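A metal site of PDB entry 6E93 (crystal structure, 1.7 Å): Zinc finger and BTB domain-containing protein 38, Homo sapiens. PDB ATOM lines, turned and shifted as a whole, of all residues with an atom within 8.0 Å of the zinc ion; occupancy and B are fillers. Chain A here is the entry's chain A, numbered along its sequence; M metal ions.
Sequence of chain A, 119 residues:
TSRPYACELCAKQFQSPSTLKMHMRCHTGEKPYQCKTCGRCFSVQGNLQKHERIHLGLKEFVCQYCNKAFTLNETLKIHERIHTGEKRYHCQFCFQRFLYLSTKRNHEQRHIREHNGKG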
ATOM      1  N   HIS A  90     -35.367  26.028  21.934  1.00  0.00           N
ATOM      2  CA  HIS A  90     -34.225  26.484  21.128  1.00  0.00           C
ATOM      3  C   HIS A  90     -33.227  27.225  22.009  1.00  0.00           C
ATOM      4  O   HIS A  90     -33.618  28.102  22.780  1.00  0.00           O
ATOM      5  CB  HIS A  90     -34.690  27.426  20.025  1.00  0.00           C
ATOM      6  CG  HIS A  90     -35.680  26.823  19.086  1.00  0.00           C
ATOM      7  ND1 HIS A  90     -36.305  25.619  19.330  1.00  0.00           N
ATOM      8  CD2 HIS A  90     -36.171  27.259  17.902  1.00  0.00           C
ATOM      9  CE1 HIS A  90     -37.131  25.334  18.340  1.00  0.00           C
ATOM     10  NE2 HIS A  90     -37.068  26.319  17.457  1.00  0.00           N
ATOM     11  N   CYS A  91     -31.938  26.872  21.905  1.00  0.00           N
ATOM     12  CA  CYS A  91     -30.944  27.734  22.520  1.00  0.00           C
ATOM     13  C   CYS A  91     -30.980  29.081  21.821  1.00  0.00           C
ATOM     14  O   CYS A  91     -31.053  29.158  20.599  1.00  0.00           O
ATOM     15  CB  CYS A  91     -29.535  27.132  22.398  1.00  0.00           C
ATOM     16  SG  CYS A  91     -28.254  28.174  23.135  1.00  0.00           S
ATOM     17  N   GLN A  92     -30.925  30.160  22.600  1.00  0.00           N
ATOM     18  CA  GLN A  92     -30.901  31.484  21.973  1.00  0.00           C
ATOM     19  C   GLN A  92     -29.541  31.876  21.436  1.00  0.00           C
ATOM     20  O   GLN A  92     -29.432  32.900  20.731  1.00  0.00           O
ATOM     21  CB  GLN A  92     -31.373  32.541  22.966  1.00  0.00           C
ATOM     22  CG  GLN A  92     -30.391  32.808  24.075  1.00  0.00           C
ATOM     23  CD  GLN A  92     -30.857  33.927  24.998  1.00  0.00           C
ATOM     24  OE1 GLN A  92     -30.718  35.096  24.683  1.00  0.00           O
ATOM     25  NE2 GLN A  92     -31.428  33.553  26.143  1.00  0.00           N
ATOM     26  N   PHE A  93     -28.481  31.105  21.733  1.00  0.00           N
ATOM     27  CA  PHE A  93     -27.145  31.480  21.319  1.00  0.00           C
ATOM     28  C   PHE A  93     -26.556  30.626  20.209  1.00  0.00           C
ATOM     29  O   PHE A  93     -25.505  31.001  19.667  1.00  0.00           O
ATOM     30  CB  PHE A  93     -26.168  31.443  22.502  1.00  0.00           C
ATOM     31  CG  PHE A  93     -26.613  32.268  23.675  1.00  0.00           C
ATOM     32  CD1 PHE A  93     -26.572  33.648  23.619  1.00  0.00           C
ATOM     33  CD2 PHE A  93     -27.052  31.655  24.817  1.00  0.00           C
ATOM     34  CE1 PHE A  93     -26.994  34.414  24.698  1.00  0.00           C
ATOM     35  CE2 PHE A  93     -27.474  32.398  25.915  1.00  0.00           C
ATOM     36  CZ  PHE A  93     -27.441  33.783  25.854  1.00  0.00           C
ATOM     37  N   CYS A  94     -27.177  29.508  19.852  1.00  0.00           N
ATOM     38  CA  CYS A  94     -26.563  28.617  18.875  1.00  0.00           C
ATOM     39  C   CYS A  94     -27.644  27.754  18.223  1.00  0.00           C
ATOM     40  O   CYS A  94     -28.831  27.857  18.542  1.00  0.00           O
ATOM     41  CB  CYS A  94     -25.470  27.759  19.530  1.00  0.00           C
ATOM     42  SG  CYS A  94     -26.043  26.306  20.440  1.00  0.00           S
ATOM     43  N   PHE A  95     -27.217  26.883  17.322  1.00  0.00           N
ATOM     44  CA  PHE A  95     -28.106  26.016  16.563  1.00  0.00           C
ATOM     45  C   PHE A  95     -28.811  24.952  17.403  1.00  0.00           C
ATOM     46  O   PHE A  95     -29.774  24.343  16.913  1.00  0.00           O
ATOM     47  CB  PHE A  95     -27.305  25.338  15.437  1.00  0.00           C
ATOM     48  CG  PHE A  95     -26.376  24.276  15.948  1.00  0.00           C
ATOM     49  CD1 PHE A  95     -25.179  24.625  16.546  1.00  0.00           C
ATOM     50  CD2 PHE A  95     -26.719  22.928  15.871  1.00  0.00           C
ATOM     51  CE1 PHE A  95     -24.302  23.642  17.050  1.00  0.00           C
ATOM     52  CE2 PHE A  95     -25.873  21.942  16.375  1.00  0.00           C
ATOM     53  CZ  PHE A  95     -24.663  22.296  16.958  1.00  0.00           C
ATOM     54  N   GLN A  96     -28.372  24.671  18.633  1.00  0.00           N
ATOM     55  CA  GLN A  96     -28.865  23.513  19.367  1.00  0.00           C
ATOM     56  C   GLN A  96     -30.343  23.643  19.740  1.00  0.00           C
ATOM     57  O   GLN A  96     -30.817  24.710  20.143  1.00  0.00           O
ATOM     58  CB  GLN A  96     -28.054  23.316  20.639  1.00  0.00           C
ATOM     59  CG  GLN A  96     -26.584  23.144  20.342  1.00  0.00           C
ATOM     60  CD  GLN A  96     -26.144  21.730  20.509  1.00  0.00           C
ATOM     61  OE1 GLN A  96     -25.271  21.438  21.323  1.00  0.00           O
ATOM     62  NE2 GLN A  96     -26.737  20.829  19.727  1.00  0.00           N
ATOM     63  N   ARG A  97     -31.055  22.521  19.618  1.00  0.00           N
ATOM     64  CA  ARG A  97     -32.481  22.430  19.936  1.00  0.00           C
ATOM     65  C   ARG A  97     -32.677  21.290  20.925  1.00  0.00           C
ATOM     66  O   ARG A  97     -31.944  20.295  20.886  1.00  0.00           O
ATOM     67  CB  ARG A  97     -33.301  22.186  18.648  1.00  0.00           C
ATOM     68  CG  ARG A  97     -33.041  23.178  17.515  1.00  0.00           C
ATOM     69  CD  ARG A  97     -33.463  24.611  17.920  1.00  0.00           C
ATOM     70  NE  ARG A  97     -33.251  25.614  16.872  1.00  0.00           N
ATOM     71  CZ  ARG A  97     -32.352  26.601  16.949  1.00  0.00           C
ATOM     72  NH1 ARG A  97     -31.575  26.695  18.026  1.00  0.00           N
ATOM     73  NH2 ARG A  97     -32.233  27.480  15.957  1.00  0.00           N
ATOM     74  N   PHE A  98     -33.657  21.436  21.826  1.00  0.00           N
ATOM     75  CA  PHE A  98     -33.803  20.472  22.918  1.00  0.00           C
ATOM     76  C   PHE A  98     -35.217  19.956  23.078  1.00  0.00           C
ATOM     77  O   PHE A  98     -36.198  20.688  22.893  1.00  0.00           O
ATOM     78  CB  PHE A  98     -33.318  21.089  24.240  1.00  0.00           C
ATOM     79  CG  PHE A  98     -31.869  21.496  24.227  1.00  0.00           C
ATOM     80  CD1 PHE A  98     -31.483  22.705  23.662  1.00  0.00           C
ATOM     81  CD2 PHE A  98     -30.894  20.648  24.697  1.00  0.00           C
ATOM     82  CE1 PHE A  98     -30.137  23.074  23.601  1.00  0.00           C
ATOM     83  CE2 PHE A  98     -29.538  21.014  24.657  1.00  0.00           C
ATOM     84  CZ  PHE A  98     -29.177  22.235  24.103  1.00  0.00           C
ATOM     85  N   LYS A 104     -32.367  22.658  27.873  1.00  0.00           N
ATOM     86  CA  LYS A 104     -32.035  23.900  27.176  1.00  0.00           C
ATOM     87  C   LYS A 104     -31.559  24.968  28.158  1.00  0.00           C
ATOM     88  O   LYS A 104     -30.563  25.662  27.894  1.00  0.00           O
ATOM     89  CB  LYS A 104     -33.247  24.391  26.390  1.00  0.00           C
ATOM     90  CG  LYS A 104     -32.940  25.617  25.528  1.00  0.00           C
ATOM     91  CD  LYS A 104     -34.123  26.559  25.509  1.00  0.00           C
ATOM     92  CE  LYS A 104     -34.049  27.508  26.646  1.00  0.00           C
ATOM     93  NZ  LYS A 104     -35.230  28.422  26.634  1.00  0.00           N
ATOM     94  N   HIS A 107     -28.051  24.351  29.269  1.00  0.00           N
ATOM     95  CA  HIS A 107     -27.106  24.570  28.169  1.00  0.00           C
ATOM     96  C   HIS A 107     -26.871  26.060  27.950  1.00  0.00           C
ATOM     97  O   HIS A 107     -25.720  26.494  27.751  1.00  0.00           O
ATOM     98  CB  HIS A 107     -27.643  23.880  26.914  1.00  0.00           C
ATOM     99  CG  HIS A 107     -27.002  24.335  25.638  1.00  0.00           C
ATOM    100  ND1 HIS A 107     -25.851  23.760  25.145  1.00  0.00           N
ATOM    101  CD2 HIS A 107     -27.382  25.270  24.731  1.00  0.00           C
ATOM    102  CE1 HIS A 107     -25.524  24.354  24.007  1.00  0.00           C
ATOM    103  NE2 HIS A 107     -26.436  25.270  23.738  1.00  0.00           N
ATOM    104  N   GLU A 108     -27.929  26.875  28.028  1.00  0.00           N
ATOM    105  CA  GLU A 108     -27.750  28.314  27.865  1.00  0.00           C
ATOM    106  C   GLU A 108     -26.874  28.888  28.968  1.00  0.00           C
ATOM    107  O   GLU A 108     -26.034  29.765  28.710  1.00  0.00           O
ATOM    108  CB  GLU A 108     -29.105  29.020  27.823  1.00  0.00           C
ATOM    109  CG  GLU A 108     -29.821  28.860  26.503  1.00  0.00           C
ATOM    110  CD  GLU A 108     -31.004  29.803  26.360  1.00  0.00           C
ATOM    111  OE1 GLU A 108     -31.234  30.618  27.281  1.00  0.00           O
ATOM    112  OE2 GLU A 108     -31.710  29.728  25.339  1.00  0.00           O
ATOM    113  N   GLN A 109     -27.056  28.400  30.200  1.00  0.00           N
ATOM    114  CA  GLN A 109     -26.246  28.875  31.323  1.00  0.00           C
ATOM    115  C   GLN A 109     -24.766  28.616  31.088  1.00  0.00           C
ATOM    116  O   GLN A 109     -23.926  29.414  31.519  1.00  0.00           O
ATOM    117  CB  GLN A 109     -26.712  28.206  32.615  1.00  0.00           C
ATOM    118  CG  GLN A 109     -27.957  28.844  33.211  1.00  0.00           C
ATOM    119  CD  GLN A 109     -27.764  30.323  33.460  1.00  0.00           C
ATOM    120  OE1 GLN A 109     -26.678  30.768  33.867  1.00  0.00           O
ATOM    121  NE2 GLN A 109     -28.811  31.106  33.220  1.00  0.00           N
ATOM    122  N   ARG A 110     -24.429  27.515  30.401  1.00  0.00           N
ATOM    123  CA  ARG A 110     -23.031  27.265  30.069  1.00  0.00           C
ATOM    124  C   ARG A 110     -22.489  28.291  29.087  1.00  0.00           C
ATOM    125  O   ARG A 110     -21.325  28.698  29.193  1.00  0.00           O
ATOM    126  CB  ARG A 110     -22.870  25.857  29.524  1.00  0.00           C
ATOM    127  CG  ARG A 110     -23.349  24.808  30.513  1.00  0.00           C
ATOM    128  CD  ARG A 110     -23.172  23.376  30.002  1.00  0.00           C
ATOM    129  NE  ARG A 110     -23.716  22.454  30.990  1.00  0.00           N
ATOM    130  CZ  ARG A 110     -24.646  21.538  30.743  1.00  0.00           C
ATOM    131  NH1 ARG A 110     -25.132  21.388  29.520  1.00  0.00           N
ATOM    132  NH2 ARG A 110     -25.071  20.751  31.729  1.00  0.00           N
ATOM    133  N   HIS A 111     -23.307  28.718  28.119  1.00  0.00           N
ATOM    134  CA  HIS A 111     -22.868  29.819  27.263  1.00  0.00           C
ATOM    135  C   HIS A 111     -22.536  31.030  28.111  1.00  0.00           C
ATOM    136  O   HIS A 111     -21.513  31.696  27.903  1.00  0.00           O
ATOM    137  CB  HIS A 111     -23.957  30.206  26.250  1.00  0.00           C
ATOM    138  CG  HIS A 111     -24.092  29.295  25.057  1.00  0.00           C
ATOM    139  ND1 HIS A 111     -23.205  29.312  24.004  1.00  0.00           N
ATOM    140  CD2 HIS A 111     -25.071  28.415  24.711  1.00  0.00           C
ATOM    141  CE1 HIS A 111     -23.605  28.452  23.076  1.00  0.00           C
ATOM    142  NE2 HIS A 111     -24.735  27.897  23.474  1.00  0.00           N
HETATM  143 ZN    ZN M   1     -26.365  26.968  22.548  1.00  0.00          ZN
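The backbone NH (N) of Gln 96 sits close to the side-chain sulfur (SG) of Cys 94. O of Cys 94 is in hydrogen-bond range of NH1 of Arg 97, at 3.0 Å. SG of Cys 91 lies close to N of Phe 93, 3.3 Å away. The backbone carbonyl oxygen of Gln 96 lies within hydrogen-bond range of the backbone NH of Cys 91, 3.0 Å away.
Four residues have an atom within 4 Å of the zinc ion: Cys 91, Cys 94, His 107 and His 111. The nearest printed residue that does not touch the zinc ion is Phe 93 (4.3 Å).
The zinc ion is bound by a ring nitrogen (NE2) of His 107, 2.1 Å away. A ring nitrogen (NE2) of His 111 is bound to the zinc ion, at 2.1 Å. The zinc ion is bound by SG of Cys 94 (2.2 Å). The side-chain sulfur (SG) of Cys 91 is bound to the zinc ion (2.3 Å).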
